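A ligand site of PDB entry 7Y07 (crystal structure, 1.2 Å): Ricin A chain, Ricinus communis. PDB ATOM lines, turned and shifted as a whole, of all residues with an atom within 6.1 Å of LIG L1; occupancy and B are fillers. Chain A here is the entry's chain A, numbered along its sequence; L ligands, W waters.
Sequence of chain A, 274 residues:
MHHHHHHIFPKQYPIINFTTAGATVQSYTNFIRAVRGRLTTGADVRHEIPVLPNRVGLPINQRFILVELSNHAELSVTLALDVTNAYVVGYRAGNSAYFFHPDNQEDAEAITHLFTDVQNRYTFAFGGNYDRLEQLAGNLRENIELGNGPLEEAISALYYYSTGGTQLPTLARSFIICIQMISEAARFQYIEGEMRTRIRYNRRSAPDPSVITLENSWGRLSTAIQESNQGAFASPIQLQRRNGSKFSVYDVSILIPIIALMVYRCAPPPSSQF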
ATOM      1  N   ASN A  85     -18.228 -11.413  20.556  1.00  0.00           N
ATOM      2  CA  ASN A  85     -18.993 -10.540  21.435  1.00  0.00           C
ATOM      3  C   ASN A  85     -19.555 -11.208  22.692  1.00  0.00           C
ATOM      4  O   ASN A  85     -20.262 -10.562  23.462  1.00  0.00           O
ATOM      5  CB  ASN A  85     -20.117  -9.846  20.643  1.00  0.00           C
ATOM      6  CG  ASN A  85     -21.002 -10.833  19.905  1.00  0.00           C
ATOM      7  OD1 ASN A  85     -20.949 -12.038  20.147  1.00  0.00           O
ATOM      8  ND2 ASN A  85     -21.829 -10.319  19.008  1.00  0.00           N
ATOM      9  N   ALA A  86     -19.234 -12.501  22.890  1.00  0.00           N
ATOM     10  CA  ALA A  86     -19.797 -13.337  23.973  1.00  0.00           C
ATOM     11  C   ALA A  86     -21.329 -13.524  23.902  1.00  0.00           C
ATOM     12  O   ALA A  86     -21.956 -13.972  24.870  1.00  0.00           O
ATOM     13  CB  ALA A  86     -19.357 -12.852  25.341  1.00  0.00           C
ATOM     14  N   TYR A  87     -21.917 -13.218  22.755  1.00  0.00           N
ATOM     15  CA  TYR A  87     -23.368 -13.272  22.549  1.00  0.00           C
ATOM     16  C   TYR A  87     -23.867 -14.715  22.554  1.00  0.00           C
ATOM     17  O   TYR A  87     -23.274 -15.577  21.899  1.00  0.00           O
ATOM     18  CB  TYR A  87     -23.706 -12.607  21.219  1.00  0.00           C
ATOM     19  CG  TYR A  87     -25.125 -12.176  21.018  1.00  0.00           C
ATOM     20  CD1 TYR A  87     -25.546 -10.882  21.370  1.00  0.00           C
ATOM     21  CD2 TYR A  87     -26.053 -13.039  20.416  1.00  0.00           C
ATOM     22  CE1 TYR A  87     -26.846 -10.477  21.156  1.00  0.00           C
ATOM     23  CE2 TYR A  87     -27.368 -12.647  20.212  1.00  0.00           C
ATOM     24  CZ  TYR A  87     -27.757 -11.369  20.584  1.00  0.00           C
ATOM     25  OH  TYR A  87     -29.051 -10.974  20.375  1.00  0.00           O
ATOM     26  N   VAL A  88     -24.935 -14.967  23.307  1.00  0.00           N
ATOM     27  CA  VAL A  88     -25.611 -16.262  23.282  1.00  0.00           C
ATOM     28  C   VAL A  88     -26.465 -16.282  22.008  1.00  0.00           C
ATOM     29  O   VAL A  88     -27.466 -15.568  21.917  1.00  0.00           O
ATOM     30  CB  VAL A  88     -26.485 -16.488  24.539  1.00  0.00           C
ATOM     31  CG1 VAL A  88     -27.203 -17.832  24.463  1.00  0.00           C
ATOM     32  CG2 VAL A  88     -25.640 -16.410  25.812  1.00  0.00           C
ATOM     33  N   VAL A  89     -26.059 -17.095  21.044  1.00  0.00           N
ATOM     34  CA  VAL A  89     -26.711 -17.129  19.723  1.00  0.00           C
ATOM     35  C   VAL A  89     -27.837 -18.165  19.634  1.00  0.00           C
ATOM     36  O   VAL A  89     -28.689 -18.090  18.748  1.00  0.00           O
ATOM     37  CB  VAL A  89     -25.712 -17.318  18.557  1.00  0.00           C
ATOM     38  CG1 VAL A  89     -24.696 -16.176  18.521  1.00  0.00           C
ATOM     39  CG2 VAL A  89     -25.007 -18.663  18.610  1.00  0.00           C
ATOM     40  N   PHE A 100     -31.567 -17.598  17.918  1.00  0.00           N
ATOM     41  CA  PHE A 100     -32.184 -16.291  17.758  1.00  0.00           C
ATOM     42  C   PHE A 100     -32.102 -15.841  16.307  1.00  0.00           C
ATOM     43  O   PHE A 100     -31.191 -16.256  15.580  1.00  0.00           O
ATOM     44  CB  PHE A 100     -31.511 -15.269  18.673  1.00  0.00           C
ATOM     45  CG  PHE A 100     -31.672 -15.561  20.140  1.00  0.00           C
ATOM     46  CD1 PHE A 100     -32.932 -15.567  20.737  1.00  0.00           C
ATOM     47  CD2 PHE A 100     -30.546 -15.835  20.932  1.00  0.00           C
ATOM     48  CE1 PHE A 100     -33.084 -15.839  22.091  1.00  0.00           C
ATOM     49  CE2 PHE A 100     -30.690 -16.102  22.285  1.00  0.00           C
ATOM     50  CZ  PHE A 100     -31.961 -16.110  22.874  1.00  0.00           C
ATOM     51  N   GLY A 128     -32.336 -11.870  19.784  1.00  0.00           N
ATOM     52  CA  GLY A 128     -31.972 -12.217  21.150  1.00  0.00           C
ATOM     53  C   GLY A 128     -31.506 -11.097  22.057  1.00  0.00           C
ATOM     54  O   GLY A 128     -30.997 -11.368  23.137  1.00  0.00           O
ATOM     55  N   ASN A 129     -31.662  -9.841  21.628  1.00  0.00           N
ATOM     56  CA  ASN A 129     -31.290  -8.701  22.455  1.00  0.00           C
ATOM     57  C   ASN A 129     -32.233  -8.528  23.646  1.00  0.00           C
ATOM     58  O   ASN A 129     -33.388  -8.971  23.601  1.00  0.00           O
ATOM     59  CB  ASN A 129     -31.236  -7.408  21.636  1.00  0.00           C
ATOM     60  CG  ASN A 129     -29.982  -7.284  20.799  1.00  0.00           C
ATOM     61  OD1 ASN A 129     -29.172  -8.215  20.698  1.00  0.00           O
ATOM     62  ND2 ASN A 129     -29.799  -6.124  20.188  1.00  0.00           N
ATOM     63  N   TYR A 130     -31.733  -7.882  24.710  1.00  0.00           N
ATOM     64  CA  TYR A 130     -32.513  -7.650  25.917  1.00  0.00           C
ATOM     65  C   TYR A 130     -33.870  -7.008  25.654  1.00  0.00           C
ATOM     66  O   TYR A 130     -34.868  -7.452  26.210  1.00  0.00           O
ATOM     67  CB  TYR A 130     -31.750  -6.800  26.939  1.00  0.00           C
ATOM     68  CG  TYR A 130     -30.576  -7.467  27.599  1.00  0.00           C
ATOM     69  CD1 TYR A 130     -30.619  -8.796  28.048  1.00  0.00           C
ATOM     70  CD2 TYR A 130     -29.407  -6.740  27.823  1.00  0.00           C
ATOM     71  CE1 TYR A 130     -29.528  -9.380  28.669  1.00  0.00           C
ATOM     72  CE2 TYR A 130     -28.312  -7.312  28.447  1.00  0.00           C
ATOM     73  CZ  TYR A 130     -28.377  -8.625  28.862  1.00  0.00           C
ATOM     74  OH  TYR A 130     -27.288  -9.185  29.481  1.00  0.00           O
ATOM     75  N   ASP A 131     -33.906  -5.961  24.806  1.00  0.00           N
ATOM     76  CA  ASP A 131     -35.174  -5.252  24.535  1.00  0.00           C
ATOM     77  C   ASP A 131     -36.280  -6.184  24.025  1.00  0.00           C
ATOM     78  O   ASP A 131     -37.395  -6.145  24.541  1.00  0.00           O
ATOM     79  CB  ASP A 131     -34.978  -4.008  23.647  1.00  0.00           C
ATOM     80  CG  ASP A 131     -34.331  -4.317  22.282  1.00  0.00           C
ATOM     81  OD1 ASP A 131     -34.032  -5.478  21.947  1.00  0.00           O
ATOM     82  OD2 ASP A 131     -34.131  -3.338  21.520  1.00  0.00           O
ATOM     83  N   LEU A 133     -36.244  -9.606  24.317  1.00  0.00           N
ATOM     84  CA  LEU A 133     -36.482 -10.628  25.342  1.00  0.00           C
ATOM     85  C   LEU A 133     -37.312 -10.112  26.515  1.00  0.00           C
ATOM     86  O   LEU A 133     -38.168 -10.826  27.024  1.00  0.00           O
ATOM     87  CB  LEU A 133     -35.163 -11.255  25.823  1.00  0.00           C
ATOM     88  CG  LEU A 133     -34.370 -12.103  24.816  1.00  0.00           C
ATOM     89  CD1 LEU A 133     -33.069 -12.548  25.470  1.00  0.00           C
ATOM     90  CD2 LEU A 133     -35.149 -13.322  24.311  1.00  0.00           C
ATOM     91  N   ARG A 141     -35.119  -6.389  32.920  1.00  0.00           N
ATOM     92  CA  ARG A 141     -34.004  -6.969  33.666  1.00  0.00           C
ATOM     93  C   ARG A 141     -34.024  -6.582  35.146  1.00  0.00           C
ATOM     94  O   ARG A 141     -33.779  -7.429  36.004  1.00  0.00           O
ATOM     95  CB  ARG A 141     -32.666  -6.577  33.051  1.00  0.00           C
ATOM     96  CG  ARG A 141     -32.255  -7.371  31.834  1.00  0.00           C
ATOM     97  CD  ARG A 141     -31.054  -6.723  31.162  1.00  0.00           C
ATOM     98  NE  ARG A 141     -31.418  -5.523  30.415  1.00  0.00           N
ATOM     99  CZ  ARG A 141     -30.605  -4.500  30.147  1.00  0.00           C
ATOM    100  NH1 ARG A 141     -29.346  -4.505  30.570  1.00  0.00           N
ATOM    101  NH2 ARG A 141     -31.050  -3.478  29.445  1.00  0.00           N
ATOM    102  N   ILE A 179     -27.996 -15.197  30.040  1.00  0.00           N
ATOM    103  CA  ILE A 179     -27.147 -14.194  29.403  1.00  0.00           C
ATOM    104  C   ILE A 179     -26.380 -13.391  30.451  1.00  0.00           C
ATOM    105  O   ILE A 179     -25.173 -13.169  30.314  1.00  0.00           O
ATOM    106  CB  ILE A 179     -27.962 -13.263  28.471  1.00  0.00           C
ATOM    107  CG1 ILE A 179     -28.479 -14.047  27.257  1.00  0.00           C
ATOM    108  CG2 ILE A 179     -27.113 -12.093  28.008  1.00  0.00           C
ATOM    109  CD1 ILE A 179     -29.710 -13.442  26.609  1.00  0.00           C
ATOM    110  N   SER A 183     -22.642 -14.538  30.044  1.00  0.00           N
ATOM    111  CA  SER A 183     -22.011 -13.549  29.169  1.00  0.00           C
ATOM    112  C   SER A 183     -21.636 -12.258  29.885  1.00  0.00           C
ATOM    113  O   SER A 183     -20.505 -11.784  29.751  1.00  0.00           O
ATOM    114  CB  SER A 183     -22.881 -13.258  27.950  1.00  0.00           C
ATOM    115  OG  SER A 183     -23.152 -14.466  27.261  1.00  0.00           O
ATOM    116  N   GLU A 184     -22.572 -11.677  30.650  1.00  0.00           N
ATOM    117  CA  GLU A 184     -22.271 -10.420  31.349  1.00  0.00           C
ATOM    118  C   GLU A 184     -21.232 -10.610  32.446  1.00  0.00           C
ATOM    119  O   GLU A 184     -20.372  -9.747  32.642  1.00  0.00           O
ATOM    120  CB  GLU A 184     -23.518  -9.728  31.896  1.00  0.00           C
ATOM    121  CG  GLU A 184     -24.571  -9.371  30.847  1.00  0.00           C
ATOM    122  CD  GLU A 184     -24.189  -8.255  29.876  1.00  0.00           C
ATOM    123  OE1 GLU A 184     -23.026  -7.812  29.822  1.00  0.00           O
ATOM    124  OE2 GLU A 184     -25.099  -7.832  29.129  1.00  0.00           O
ATOM    125  N   ARG A 187     -17.940 -10.717  30.783  1.00  0.00           N
ATOM    126  CA  ARG A 187     -17.559  -9.374  30.340  1.00  0.00           C
ATOM    127  C   ARG A 187     -17.061  -8.479  31.478  1.00  0.00           C
ATOM    128  O   ARG A 187     -16.159  -7.668  31.271  1.00  0.00           O
ATOM    129  CB  ARG A 187     -18.706  -8.676  29.619  1.00  0.00           C
ATOM    130  CG  ARG A 187     -19.071  -9.252  28.269  1.00  0.00           C
ATOM    131  CD  ARG A 187     -20.405  -8.699  27.798  1.00  0.00           C
ATOM    132  NE  ARG A 187     -20.863  -9.366  26.588  1.00  0.00           N
ATOM    133  CZ  ARG A 187     -22.125  -9.691  26.316  1.00  0.00           C
ATOM    134  NH1 ARG A 187     -23.096  -9.406  27.173  1.00  0.00           N
ATOM    135  NH2 ARG A 187     -22.418 -10.301  25.185  1.00  0.00           N
ATOM    136  N   GLU A 215     -24.041  -3.352  31.944  1.00  0.00           N
ATOM    137  CA  GLU A 215     -24.524  -4.132  30.788  1.00  0.00           C
ATOM    138  C   GLU A 215     -24.834  -3.229  29.596  1.00  0.00           C
ATOM    139  O   GLU A 215     -24.373  -3.482  28.473  1.00  0.00           O
ATOM    140  CB  GLU A 215     -25.774  -4.931  31.162  1.00  0.00           C
ATOM    141  CG  GLU A 215     -25.528  -5.991  32.218  1.00  0.00           C
ATOM    142  CD  GLU A 215     -26.781  -6.678  32.694  1.00  0.00           C
ATOM    143  OE1 GLU A 215     -27.895  -6.306  32.267  1.00  0.00           O
ATOM    144  OE2 GLU A 215     -26.650  -7.611  33.517  1.00  0.00           O
ATOM    145  N   ASN A 216     -25.569  -2.157  29.857  1.00  0.00           N
ATOM    146  CA  ASN A 216     -25.957  -1.190  28.833  1.00  0.00           C
ATOM    147  C   ASN A 216     -24.787  -0.423  28.240  1.00  0.00           C
ATOM    148  O   ASN A 216     -24.883   0.071  27.123  1.00  0.00           O
ATOM    149  CB  ASN A 216     -26.987  -0.212  29.397  1.00  0.00           C
ATOM    150  CG  ASN A 216     -28.316  -0.874  29.726  1.00  0.00           C
ATOM    151  OD1 ASN A 216     -28.563  -2.028  29.383  1.00  0.00           O
ATOM    152  ND2 ASN A 216     -29.176  -0.127  30.411  1.00  0.00           N
ATOM    153  N   SER A 217     -23.683  -0.340  28.984  1.00  0.00           N
ATOM    154  CA  SER A 217     -22.538   0.458  28.590  1.00  0.00           C
ATOM    155  C   SER A 217     -21.359  -0.337  28.022  1.00  0.00           C
ATOM    156  O   SER A 217     -20.352   0.263  27.678  1.00  0.00           O
ATOM    157  CB  SER A 217     -22.049   1.291  29.773  1.00  0.00           C
ATOM    158  OG  SER A 217     -23.083   2.111  30.274  1.00  0.00           O
HETATM  159  C1  LIG L   1     -27.885 -12.393  23.856  1.00  0.00           C
HETATM  160  C2  LIG L   1     -25.841 -11.625  24.902  1.00  0.00           C
HETATM  161  N1  LIG L   1     -28.379 -11.148  23.928  1.00  0.00           N
HETATM  162  C3  LIG L   1     -26.287  -8.028  25.480  1.00  0.00           C
HETATM  163  N2  LIG L   1     -28.602 -13.381  23.328  1.00  0.00           N
HETATM  164  O1  LIG L   1     -24.722 -11.886  25.334  1.00  0.00           O
HETATM  165  C4  LIG L   1     -27.576  -7.837  24.965  1.00  0.00           C
HETATM  166  C5  LIG L   1     -28.790  -1.362  26.242  1.00  0.00           C
HETATM  167  C6  LIG L   1     -29.240  -0.042  26.125  1.00  0.00           C
HETATM  168  C7  LIG L   1     -28.502   0.886  25.379  1.00  0.00           C
HETATM  169  C8  LIG L   1     -27.305   0.500  24.750  1.00  0.00           C
HETATM  170  C9  LIG L   1     -26.864  -0.825  24.868  1.00  0.00           C
HETATM  171  C10 LIG L   1     -27.598  -1.761  25.610  1.00  0.00           C
HETATM  172  C11 LIG L   1     -27.133  -3.087  25.733  1.00  0.00           C
HETATM  173  C12 LIG L   1     -27.951  -4.113  24.891  1.00  0.00           C
HETATM  174  C13 LIG L   1     -27.926  -3.768  23.385  1.00  0.00           C
HETATM  175  O2  LIG L   1     -26.616  -3.987  22.853  1.00  0.00           O
HETATM  176  N3  LIG L   1     -27.433  -5.490  25.082  1.00  0.00           N
HETATM  177  C14 LIG L   1     -28.207  -6.581  24.898  1.00  0.00           C
HETATM  178  O3  LIG L   1     -29.358  -6.506  24.455  1.00  0.00           O
HETATM  179  N4  LIG L   1     -28.223  -8.904  24.449  1.00  0.00           N
HETATM  180  C15 LIG L   1     -27.674 -10.122  24.439  1.00  0.00           C
HETATM  181  N5  LIG L   1     -26.608 -12.666  24.346  1.00  0.00           N
HETATM  182  C16 LIG L   1     -26.385 -10.334  24.947  1.00  0.00           C
HETATM  183  N6  LIG L   1     -25.706  -9.301  25.466  1.00  0.00           N
HETATM  184  C1  LG2 L   2     -24.442 -12.471  17.076  1.00  0.00           C
HETATM  185  C2  LG2 L   2     -26.792 -11.966  16.812  1.00  0.00           C
HETATM  186  N1  LG2 L   2     -24.226 -11.254  17.596  1.00  0.00           N
HETATM  187  C3  LG2 L   2     -27.273  -8.539  18.041  1.00  0.00           C
HETATM  188  N2  LG2 L   2     -23.443 -13.332  16.946  1.00  0.00           N
HETATM  189  O1  LG2 L   2     -27.915 -12.297  16.453  1.00  0.00           O
HETATM  190  C4  LG2 L   2     -25.962  -8.212  18.423  1.00  0.00           C
HETATM  191  C5  LG2 L   2     -22.809  -7.404  21.554  1.00  0.00           C
HETATM  192  C6  LG2 L   2     -23.081  -8.017  22.777  1.00  0.00           C
HETATM  193  C7  LG2 L   2     -23.447  -7.245  23.880  1.00  0.00           C
HETATM  194  C8  LG2 L   2     -23.560  -5.849  23.767  1.00  0.00           C
HETATM  195  C9  LG2 L   2     -23.290  -5.234  22.535  1.00  0.00           C
HETATM  196  C10 LG2 L   2     -22.926  -6.002  21.423  1.00  0.00           C
HETATM  197  C11 LG2 L   2     -22.665  -5.391  20.192  1.00  0.00           C
HETATM  198  C12 LG2 L   2     -23.954  -5.216  19.359  1.00  0.00           C
HETATM  199  C13 LG2 L   2     -23.719  -4.234  18.203  1.00  0.00           C
HETATM  200  O2  LG2 L   2     -22.879  -4.822  17.198  1.00  0.00           O
HETATM  201  N3  LG2 L   2     -24.428  -6.523  18.855  1.00  0.00           N
HETATM  202  C14 LG2 L   2     -25.701  -6.952  18.958  1.00  0.00           C
HETATM  203  O3  LG2 L   2     -26.611  -6.268  19.451  1.00  0.00           O
HETATM  204  N4  LG2 L   2     -24.977  -9.130  18.266  1.00  0.00           N
HETATM  205  C15 LG2 L   2     -25.234 -10.356  17.741  1.00  0.00           C
HETATM  206  N5  LG2 L   2     -25.727 -12.863  16.678  1.00  0.00           N
HETATM  207  C16 LG2 L   2     -26.536 -10.699  17.352  1.00  0.00           C
HETATM  208  N6  LG2 L   2     -27.537  -9.811  17.502  1.00  0.00           N
HETATM  209  O   HOH W   1     -31.417  -4.577  23.838  1.00  0.00           O
HETATM  210  O   HOH W   2     -26.464  -6.752  22.229  1.00  0.00           O
HETATM  211  O   HOH W   3     -25.199  -5.782  27.197  1.00  0.00           O
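O of Gly 128 is in hydrogen-bond range of N2 of LIG L1 (3.1 Å).
N of Tyr 130 is in hydrogen-bond range of O3 of LIG L1 (2.8 Å).
O1 of LIG L1 sits at hydrogen-bond distance from NH2 of Arg 187 (2.8 Å).
The backbone carbonyl oxygen (O) of Val 88 is in hydrogen-bond range of a nitrogen (N2) of LIG L1 (2.8 Å).
The side-chain hydroxyl of Tyr 87 is in hydrogen-bond range of a nitrogen (N6) of LG2 L2 (3.4 Å).
ND2 of Asn 129 sits at hydrogen-bond distance from O3 of LG2 L2 (3.3 Å).
A nitrogen (N1) of LG2 L2 lies within hydrogen-bond range of the side-chain amide nitrogen (ND2) of Asn 85 (2.9 Å).
The backbone carbonyl oxygen (O) of Gly 128 sits close to the side-chain hydroxyl (OH) of Tyr 87, at 3.4 Å.
OH of Tyr 130 is in hydrogen-bond range of OE2 of Glu 184, 2.6 Å away.
NH1 of Arg 187 is in salt-bridge range of OE1 of Glu 184 (3.1 Å).
OD1 of Asn 216 lies within hydrogen-bond range of NH1 of Arg 141 (2.9 Å).
OH of Tyr 87 is in hydrogen-bond range of OD1 of Asn 129, at 2.8 Å.
OD1 of Asn 85 sits close to N of Tyr 87 (3.0 Å).
O of Ala 86 lies within hydrogen-bond range of OG of Ser 183, 2.7 Å away.
The side-chain carboxylate (OE1) of Glu 215 lies within salt-bridge range of the guanidinium group (NH1) of Arg 141, at 2.9 Å.
O1 of LIG L1 lies close to O of Ala 86.
Merely in contact with LIG L1: Asn 216 (3.1 Å), Tyr 87 (3.2 Å), Ile 179 (3.4 Å), Ser 183 (3.5 Å), Asn 129 (3.5 Å), Phe 100 (3.6 Å), Glu 184 (3.8 Å) and Glu 215 (3.9 Å).
Hydrophobic or aromatic side chains within 4 Å of LIG L1: Tyr 87, Val 88, Phe 100, Tyr 130 and Ile 179.
Within 4 Å of LIG L1: Ala 86, Tyr 87, Val 88, Phe 100, Gly 128, Asn 129, Tyr 130, Ile 179, Ser 183, Glu 184, Arg 187, Glu 215 and Asn 216.
Water W2 lies within hydrogen-bond range of an oxygen (O3) of LG2 L2, an oxygen (O2) of LIG L1 and the side-chain amide oxygen of Asn 129.
Water W1 lies within hydrogen-bond range of O3 of LIG L1 (2.9 Å), N of Asp 131 (3.0 Å) and N of Tyr 130 (3.4 Å).
Water W3 lies within hydrogen-bond range of O of Glu 215, OE2 of Glu 184 and N3 of LIG L1.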
